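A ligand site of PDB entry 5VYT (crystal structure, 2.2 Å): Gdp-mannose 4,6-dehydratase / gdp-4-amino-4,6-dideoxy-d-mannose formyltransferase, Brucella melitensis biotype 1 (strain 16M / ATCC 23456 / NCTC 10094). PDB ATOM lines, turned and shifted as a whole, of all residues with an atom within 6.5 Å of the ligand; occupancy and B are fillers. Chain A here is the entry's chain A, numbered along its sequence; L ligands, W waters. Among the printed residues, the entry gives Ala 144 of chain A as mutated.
N2 of the ligand is in hydrogen-bond range of O of Asp 141, at 2.8 Å. A nitrogen (N1) of the ligand sits at hydrogen-bond distance from the backbone NH of Ile 93, at 3.3 Å. The backbone NH (N) of Asp 145 lies within hydrogen-bond range of an oxygen (O1) of the ligand (2.8 Å). The backbone carbonyl oxygen of Asn 143 lies close to a nitrogen (N3) of the ligand. An oxygen (O2) of the ligand sits close to the side-chain amide nitrogen (ND2) of Asn 107. A nitrogen (N5) of the ligand sits at hydrogen-bond distance from the backbone carbonyl oxygen of Ser 91, 2.8 Å away. The backbone carbonyl oxygen (O) of Ile 93 lies within hydrogen-bond range of a nitrogen (N2) of the ligand (3.0 Å).
The backbone carbonyl oxygen (O) of His 138 sits at hydrogen-bond distance from the backbone NH (N) of Asn 107 (2.7 Å). OD1 of Asn 107 sits at hydrogen-bond distance from OG of Ser 86, 2.6 Å away. The side-chain hydroxyl (OG1) of Thr 146 sits close to the side-chain carboxylate (OD2) of Asp 141 (3.4 Å). A ring nitrogen (ND1) of His 138 sits at hydrogen-bond distance from the backbone carbonyl oxygen of Thr 146 (3.2 Å). The backbone NH of Gly 118 lies within hydrogen-bond range of the side-chain carboxylate of Asp 145, 3.0 Å away. OD1 of Asp 141 sits close to N of Asn 143. N of Arg 203 sits close to OG1 of Thr 119, at 3.5 Å. The side-chain hydroxyl of Thr 146 sits close to the backbone carbonyl oxygen of Asn 143 (3.3 Å).
Tyr 89 touches the ligand. Arg 90 touches the ligand. CD1 of Leu 92 touches N1 of the ligand, 3.5 Å away. Leu 98 touches the ligand (CD1 to N2, 3.8 Å). CE1 of His 138 touches O1 of the ligand (3.9 Å). Met 140 touches the ligand. Glu 142 touches the ligand. CA of Ala 144 touches O1 of the ligand (3.5 Å). Arg 203 touches the ligand. Hydrophobic or aromatic side chains within 4 Å of the ligand: Leu 92, Ile 93, Leu 98, His 138 and Met 140. 15 residues have an atom within 4 Å of the ligand: Tyr 89, Arg 90, Ser 91, Leu 92, Ile 93, Leu 98, Asn 107, His 138, Met 140, Asp 141, Glu 142, Asn 143, Ala 144, Asp 145 and Arg 203.
Water W1 lies within hydrogen-bond range of the backbone carbonyl oxygen (O) of Asn 143 (2.6 Å), the backbone carbonyl oxygen (O) of Thr 146 (2.9 Å), the backbone NH (N) of Asp 141 (3.0 Å) and a nitrogen (N3) of the ligand (3.0 Å).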
ATOM      1  N   SER A  86      28.009  -8.159   2.398  1.00  0.00           N
ATOM      2  CA  SER A  86      28.716  -6.954   1.926  1.00  0.00           C
ATOM      3  C   SER A  86      29.017  -5.974   3.086  1.00  0.00           C
ATOM      4  O   SER A  86      28.096  -5.401   3.715  1.00  0.00           O
ATOM      5  CB  SER A  86      27.913  -6.259   0.823  1.00  0.00           C
ATOM      6  OG  SER A  86      28.389  -4.967   0.554  1.00  0.00           O
ATOM      7  N   HIS A  88      31.023  -2.721   3.501  1.00  0.00           N
ATOM      8  CA  HIS A  88      31.731  -1.573   2.916  1.00  0.00           C
ATOM      9  C   HIS A  88      32.445  -1.934   1.624  1.00  0.00           C
ATOM     10  O   HIS A  88      33.520  -1.423   1.320  1.00  0.00           O
ATOM     11  CB  HIS A  88      32.724  -0.975   3.934  1.00  0.00           C
ATOM     12  CG  HIS A  88      32.064  -0.196   5.026  1.00  0.00           C
ATOM     13  ND1 HIS A  88      32.673   0.891   5.632  1.00  0.00           N
ATOM     14  CD2 HIS A  88      30.853  -0.323   5.600  1.00  0.00           C
ATOM     15  CE1 HIS A  88      31.858   1.386   6.536  1.00  0.00           C
ATOM     16  NE2 HIS A  88      30.742   0.672   6.544  1.00  0.00           N
ATOM     17  N   TYR A  89      31.864  -2.848   0.862  1.00  0.00           N
ATOM     18  CA  TYR A  89      32.406  -3.186  -0.432  1.00  0.00           C
ATOM     19  C   TYR A  89      32.052  -1.974  -1.314  1.00  0.00           C
ATOM     20  O   TYR A  89      30.946  -1.465  -1.254  1.00  0.00           O
ATOM     21  CB  TYR A  89      31.852  -4.546  -0.949  1.00  0.00           C
ATOM     22  CG  TYR A  89      32.544  -5.067  -2.181  1.00  0.00           C
ATOM     23  CD1 TYR A  89      33.786  -5.701  -2.107  1.00  0.00           C
ATOM     24  CD2 TYR A  89      31.964  -4.924  -3.423  1.00  0.00           C
ATOM     25  CE1 TYR A  89      34.426  -6.172  -3.250  1.00  0.00           C
ATOM     26  CE2 TYR A  89      32.575  -5.375  -4.572  1.00  0.00           C
ATOM     27  CZ  TYR A  89      33.801  -6.010  -4.486  1.00  0.00           C
ATOM     28  OH  TYR A  89      34.420  -6.431  -5.656  1.00  0.00           O
ATOM     29  N   ARG A  90      33.029  -1.502  -2.074  1.00  0.00           N
ATOM     30  CA  ARG A  90      32.963  -0.206  -2.789  1.00  0.00           C
ATOM     31  C   ARG A  90      32.464  -0.282  -4.239  1.00  0.00           C
ATOM     32  O   ARG A  90      32.380   0.755  -4.901  1.00  0.00           O
ATOM     33  CB  ARG A  90      34.341   0.457  -2.754  1.00  0.00           C
ATOM     34  CG  ARG A  90      34.917   0.615  -1.343  1.00  0.00           C
ATOM     35  CD  ARG A  90      36.330   1.180  -1.319  1.00  0.00           C
ATOM     36  NE  ARG A  90      36.348   2.622  -1.589  1.00  0.00           N
ATOM     37  CZ  ARG A  90      36.027   3.573  -0.710  1.00  0.00           C
ATOM     38  NH1 ARG A  90      35.687   3.302   0.550  1.00  0.00           N
ATOM     39  NH2 ARG A  90      36.066   4.845  -1.112  1.00  0.00           N
ATOM     40  N   SER A  91      32.088  -1.476  -4.708  1.00  0.00           N
ATOM     41  CA  SER A  91      31.610  -1.648  -6.082  1.00  0.00           C
ATOM     42  C   SER A  91      30.323  -2.456  -6.142  1.00  0.00           C
ATOM     43  O   SER A  91      30.106  -3.367  -5.358  1.00  0.00           O
ATOM     44  CB  SER A  91      32.642  -2.351  -6.954  1.00  0.00           C
ATOM     45  OG  SER A  91      33.872  -1.682  -6.869  1.00  0.00           O
ATOM     46  N   LEU A  92      29.502  -2.123  -7.128  1.00  0.00           N
ATOM     47  CA  LEU A  92      28.222  -2.766  -7.322  1.00  0.00           C
ATOM     48  C   LEU A  92      28.480  -4.201  -7.717  1.00  0.00           C
ATOM     49  O   LEU A  92      29.297  -4.486  -8.579  1.00  0.00           O
ATOM     50  CB  LEU A  92      27.422  -2.051  -8.401  1.00  0.00           C
ATOM     51  CG  LEU A  92      25.905  -2.215  -8.304  1.00  0.00           C
ATOM     52  CD1 LEU A  92      25.329  -1.492  -7.074  1.00  0.00           C
ATOM     53  CD2 LEU A  92      25.290  -1.674  -9.592  1.00  0.00           C
ATOM     54  N   ILE A  93      27.779  -5.085  -7.040  1.00  0.00           N
ATOM     55  CA  ILE A  93      27.884  -6.483  -7.193  1.00  0.00           C
ATOM     56  C   ILE A  93      26.718  -6.837  -8.119  1.00  0.00           C
ATOM     57  O   ILE A  93      25.547  -6.633  -7.738  1.00  0.00           O
ATOM     58  CB  ILE A  93      27.758  -7.194  -5.821  1.00  0.00           C
ATOM     59  CG1 ILE A  93      28.837  -6.701  -4.883  1.00  0.00           C
ATOM     60  CG2 ILE A  93      27.886  -8.698  -5.969  1.00  0.00           C
ATOM     61  CD1 ILE A  93      28.847  -7.413  -3.544  1.00  0.00           C
ATOM     62  N   PRO A  94      27.022  -7.364  -9.336  1.00  0.00           N
ATOM     63  CA  PRO A  94      25.989  -7.711 -10.317  1.00  0.00           C
ATOM     64  C   PRO A  94      25.020  -8.701  -9.779  1.00  0.00           C
ATOM     65  O   PRO A  94      25.383  -9.521  -8.930  1.00  0.00           O
ATOM     66  CB  PRO A  94      26.765  -8.407 -11.425  1.00  0.00           C
ATOM     67  CG  PRO A  94      28.113  -7.876 -11.340  1.00  0.00           C
ATOM     68  CD  PRO A  94      28.373  -7.588  -9.882  1.00  0.00           C
ATOM     69  N   GLY A  95      23.814  -8.662 -10.311  1.00  0.00           N
ATOM     70  CA  GLY A  95      22.756  -9.574  -9.933  1.00  0.00           C
ATOM     71  C   GLY A  95      23.141 -11.049 -10.090  1.00  0.00           C
ATOM     72  O   GLY A  95      22.886 -11.855  -9.190  1.00  0.00           O
ATOM     73  N   LEU A  98      25.066 -12.120  -7.019  1.00  0.00           N
ATOM     74  CA  LEU A  98      24.184 -12.232  -5.830  1.00  0.00           C
ATOM     75  C   LEU A  98      23.310 -13.495  -5.897  1.00  0.00           C
ATOM     76  O   LEU A  98      23.014 -14.111  -4.876  1.00  0.00           O
ATOM     77  CB  LEU A  98      23.273 -11.017  -5.746  1.00  0.00           C
ATOM     78  CG  LEU A  98      23.918  -9.648  -5.452  1.00  0.00           C
ATOM     79  CD1 LEU A  98      22.815  -8.581  -5.364  1.00  0.00           C
ATOM     80  CD2 LEU A  98      24.747  -9.673  -4.168  1.00  0.00           C
ATOM     81  N   ASN A 107      23.734  -6.295   2.988  1.00  0.00           N
ATOM     82  CA  ASN A 107      24.648  -5.179   2.903  1.00  0.00           C
ATOM     83  C   ASN A 107      24.496  -4.280   4.135  1.00  0.00           C
ATOM     84  O   ASN A 107      23.365  -4.139   4.640  1.00  0.00           O
ATOM     85  CB  ASN A 107      24.353  -4.313   1.694  1.00  0.00           C
ATOM     86  CG  ASN A 107      25.327  -3.158   1.594  1.00  0.00           C
ATOM     87  OD1 ASN A 107      26.515  -3.364   1.364  1.00  0.00           O
ATOM     88  ND2 ASN A 107      24.854  -1.957   1.878  1.00  0.00           N
ATOM     89  N   LEU A 108      25.571  -3.622   4.562  1.00  0.00           N
ATOM     90  CA  LEU A 108      25.464  -2.605   5.623  1.00  0.00           C
ATOM     91  C   LEU A 108      25.361  -1.218   5.023  1.00  0.00           C
ATOM     92  O   LEU A 108      26.275  -0.803   4.362  1.00  0.00           O
ATOM     93  CB  LEU A 108      26.669  -2.625   6.550  1.00  0.00           C
ATOM     94  CG  LEU A 108      26.666  -1.596   7.695  1.00  0.00           C
ATOM     95  CD1 LEU A 108      25.366  -1.641   8.504  1.00  0.00           C
ATOM     96  CD2 LEU A 108      27.866  -1.863   8.607  1.00  0.00           C
ATOM     97  N   HIS A 109      24.265  -0.500   5.264  1.00  0.00           N
ATOM     98  CA  HIS A 109      24.209   0.913   4.846  1.00  0.00           C
ATOM     99  C   HIS A 109      24.020   1.863   6.028  1.00  0.00           C
ATOM    100  O   HIS A 109      23.126   1.646   6.829  1.00  0.00           O
ATOM    101  CB  HIS A 109      23.111   1.147   3.830  1.00  0.00           C
ATOM    102  CG  HIS A 109      23.259   2.437   3.091  1.00  0.00           C
ATOM    103  ND1 HIS A 109      22.470   3.532   3.343  1.00  0.00           N
ATOM    104  CD2 HIS A 109      24.156   2.811   2.149  1.00  0.00           C
ATOM    105  CE1 HIS A 109      22.832   4.519   2.550  1.00  0.00           C
ATOM    106  NE2 HIS A 109      23.869   4.119   1.824  1.00  0.00           N
ATOM    107  N   GLY A 118      22.795   6.383  -1.329  1.00  0.00           N
ATOM    108  CA  GLY A 118      23.914   6.956  -2.046  1.00  0.00           C
ATOM    109  C   GLY A 118      25.134   6.904  -1.172  1.00  0.00           C
ATOM    110  O   GLY A 118      25.306   5.955  -0.388  1.00  0.00           O
ATOM    111  N   THR A 119      25.977   7.936  -1.299  1.00  0.00           N
ATOM    112  CA  THR A 119      27.219   8.049  -0.554  1.00  0.00           C
ATOM    113  C   THR A 119      27.213   9.376   0.221  1.00  0.00           C
ATOM    114  O   THR A 119      26.207  10.120   0.205  1.00  0.00           O
ATOM    115  CB  THR A 119      28.437   7.945  -1.518  1.00  0.00           C
ATOM    116  OG1 THR A 119      28.369   9.002  -2.497  1.00  0.00           O
ATOM    117  CG2 THR A 119      28.460   6.600  -2.237  1.00  0.00           C
ATOM    118  N   HIS A 138      20.529  -4.655   4.982  1.00  0.00           N
ATOM    119  CA  HIS A 138      19.486  -5.034   4.057  1.00  0.00           C
ATOM    120  C   HIS A 138      19.895  -6.087   3.047  1.00  0.00           C
ATOM    121  O   HIS A 138      21.066  -6.157   2.662  1.00  0.00           O
ATOM    122  CB  HIS A 138      18.941  -3.795   3.340  1.00  0.00           C
ATOM    123  CG  HIS A 138      19.932  -3.158   2.440  1.00  0.00           C
ATOM    124  ND1 HIS A 138      20.021  -3.471   1.104  1.00  0.00           N
ATOM    125  CD2 HIS A 138      20.914  -2.279   2.683  1.00  0.00           C
ATOM    126  CE1 HIS A 138      20.986  -2.771   0.548  1.00  0.00           C
ATOM    127  NE2 HIS A 138      21.552  -2.038   1.484  1.00  0.00           N
ATOM    128  N   MET A 140      20.204  -7.521  -0.627  1.00  0.00           N
ATOM    129  CA  MET A 140      20.597  -6.826  -1.855  1.00  0.00           C
ATOM    130  C   MET A 140      19.863  -7.310  -3.104  1.00  0.00           C
ATOM    131  O   MET A 140      19.461  -8.457  -3.211  1.00  0.00           O
ATOM    132  CB  MET A 140      22.105  -6.972  -2.086  1.00  0.00           C
ATOM    133  CG  MET A 140      22.971  -6.055  -1.242  1.00  0.00           C
ATOM    134  SD  MET A 140      24.760  -6.216  -1.561  1.00  0.00           S
ATOM    135  CE  MET A 140      25.041  -7.741  -0.694  1.00  0.00           C
ATOM    136  N   ASP A 141      19.712  -6.407  -4.058  1.00  0.00           N
ATOM    137  CA  ASP A 141      19.350  -6.810  -5.410  1.00  0.00           C
ATOM    138  C   ASP A 141      20.339  -6.148  -6.384  1.00  0.00           C
ATOM    139  O   ASP A 141      21.322  -5.584  -5.958  1.00  0.00           O
ATOM    140  CB  ASP A 141      17.882  -6.503  -5.712  1.00  0.00           C
ATOM    141  CG  ASP A 141      17.481  -5.109  -5.282  1.00  0.00           C
ATOM    142  OD1 ASP A 141      18.246  -4.161  -5.589  1.00  0.00           O
ATOM    143  OD2 ASP A 141      16.413  -5.004  -4.615  1.00  0.00           O
ATOM    144  N   GLU A 142      20.090  -6.282  -7.682  1.00  0.00           N
ATOM    145  CA  GLU A 142      20.964  -5.713  -8.693  1.00  0.00           C
ATOM    146  C   GLU A 142      21.162  -4.214  -8.528  1.00  0.00           C
ATOM    147  O   GLU A 142      22.186  -3.706  -8.926  1.00  0.00           O
ATOM    148  CB  GLU A 142      20.497  -6.086 -10.126  1.00  0.00           C
ATOM    149  CG  GLU A 142      19.157  -5.521 -10.640  1.00  0.00           C
ATOM    150  CD  GLU A 142      17.911  -6.321 -10.224  1.00  0.00           C
ATOM    151  OE1 GLU A 142      18.024  -7.234  -9.364  1.00  0.00           O
ATOM    152  OE2 GLU A 142      16.812  -6.009 -10.767  1.00  0.00           O
ATOM    153  N   ASN A 143      20.225  -3.523  -7.892  1.00  0.00           N
ATOM    154  CA  ASN A 143      20.313  -2.083  -7.628  1.00  0.00           C
ATOM    155  C   ASN A 143      21.011  -1.681  -6.316  1.00  0.00           C
ATOM    156  O   ASN A 143      21.267  -2.506  -5.447  1.00  0.00           O
ATOM    157  CB  ASN A 143      18.904  -1.491  -7.686  1.00  0.00           C
ATOM    158  CG  ASN A 143      18.287  -1.668  -9.035  1.00  0.00           C
ATOM    159  OD1 ASN A 143      18.779  -1.106 -10.002  1.00  0.00           O
ATOM    160  ND2 ASN A 143      17.254  -2.494  -9.130  1.00  0.00           N
ATOM    161  N   ALA A 144      21.331  -0.403  -6.190  1.00  0.00           N
ATOM    162  CA  ALA A 144      22.037   0.106  -5.016  1.00  0.00           C
ATOM    163  C   ALA A 144      21.012   0.507  -3.949  1.00  0.00           C
ATOM    164  O   ALA A 144      20.005   1.133  -4.250  1.00  0.00           O
ATOM    165  CB  ALA A 144      22.944   1.275  -5.376  1.00  0.00           C
ATOM    166  N   ASP A 145      21.274   0.071  -2.709  1.00  0.00           N
ATOM    167  CA  ASP A 145      20.547   0.500  -1.483  1.00  0.00           C
ATOM    168  C   ASP A 145      19.083   0.106  -1.440  1.00  0.00           C
ATOM    169  O   ASP A 145      18.326   0.605  -0.575  1.00  0.00           O
ATOM    170  CB  ASP A 145      20.732   2.015  -1.247  1.00  0.00           C
ATOM    171  CG  ASP A 145      22.198   2.440  -1.230  1.00  0.00           C
ATOM    172  OD1 ASP A 145      23.045   1.748  -0.618  1.00  0.00           O
ATOM    173  OD2 ASP A 145      22.506   3.472  -1.849  1.00  0.00           O
ATOM    174  N   THR A 146      18.696  -0.801  -2.325  1.00  0.00           N
ATOM    175  CA  THR A 146      17.358  -1.375  -2.400  1.00  0.00           C
ATOM    176  C   THR A 146      17.362  -2.769  -1.733  1.00  0.00           C
ATOM    177  O   THR A 146      18.411  -3.433  -1.607  1.00  0.00           O
ATOM    178  CB  THR A 146      16.935  -1.561  -3.873  1.00  0.00           C
ATOM    179  OG1 THR A 146      18.073  -2.028  -4.618  1.00  0.00           O
ATOM    180  CG2 THR A 146      16.459  -0.240  -4.496  1.00  0.00           C
ATOM    181  N   ARG A 203      28.147  10.934  -5.368  1.00  0.00           N
ATOM    182  CA  ARG A 203      29.589  10.744  -5.147  1.00  0.00           C
ATOM    183  C   ARG A 203      30.202  12.033  -4.604  1.00  0.00           C
ATOM    184  O   ARG A 203      30.752  12.060  -3.497  1.00  0.00           O
ATOM    185  CB  ARG A 203      30.309  10.378  -6.485  1.00  0.00           C
ATOM    186  CG  ARG A 203      31.591   9.565  -6.351  1.00  0.00           C
ATOM    187  CD  ARG A 203      31.305   8.077  -6.269  1.00  0.00           C
ATOM    188  NE  ARG A 203      31.878   7.476  -5.067  1.00  0.00           N
ATOM    189  CZ  ARG A 203      31.561   6.280  -4.551  1.00  0.00           C
ATOM    190  NH1 ARG A 203      30.662   5.459  -5.129  1.00  0.00           N
ATOM    191  NH2 ARG A 203      32.176   5.876  -3.428  1.00  0.00           N
HETATM  192  N1  LIG L   1      25.802  -3.989  -4.695  1.00  0.00           N
HETATM  193  C1  LIG L   1      24.485  -4.121  -4.800  1.00  0.00           C
HETATM  194  N2  LIG L   1      24.008  -5.016  -5.710  1.00  0.00           N
HETATM  195  N3  LIG L   1      23.650  -3.407  -4.011  1.00  0.00           N
HETATM  196  C2  LIG L   1      24.139  -2.520  -3.101  1.00  0.00           C
HETATM  197  O1  LIG L   1      23.305  -1.891  -2.427  1.00  0.00           O
HETATM  198  C3  LIG L   1      25.634  -2.357  -2.944  1.00  0.00           C
HETATM  199  N4  LIG L   1      26.365  -1.465  -2.104  1.00  0.00           N
HETATM  200  C4  LIG L   1      27.647  -0.878  -2.614  1.00  0.00           C
HETATM  201  C5  LIG L   1      28.454  -2.131  -2.945  1.00  0.00           C
HETATM  202  N5  LIG L   1      27.767  -3.091  -3.817  1.00  0.00           N
HETATM  203  C6  LIG L   1      26.422  -3.186  -3.851  1.00  0.00           C
HETATM  204  C7  LIG L   1      27.278   0.116  -3.758  1.00  0.00           C
HETATM  205  N6  LIG L   1      28.352   0.741  -4.536  1.00  0.00           N
HETATM  206  C8  LIG L   1      27.854   3.156  -8.038  1.00  0.00           C
HETATM  207  C9  LIG L   1      26.744   2.751  -7.271  1.00  0.00           C
HETATM  208  C10 LIG L   1      26.883   1.954  -6.107  1.00  0.00           C
HETATM  209  C11 LIG L   1      28.151   1.539  -5.649  1.00  0.00           C
HETATM  210  C12 LIG L   1      29.248   1.952  -6.433  1.00  0.00           C
HETATM  211  C13 LIG L   1      29.117   2.749  -7.602  1.00  0.00           C
HETATM  212  C14 LIG L   1      25.950  -1.142  -0.965  1.00  0.00           C
HETATM  213  O2  LIG L   1      26.561  -0.367  -0.245  1.00  0.00           O
HETATM  214  O   HOH W   1      20.827  -3.804  -3.187  1.00  0.00           O
HETATM  215  O   HOH W   2      30.568  -0.062  -8.918  1.00  0.00           O
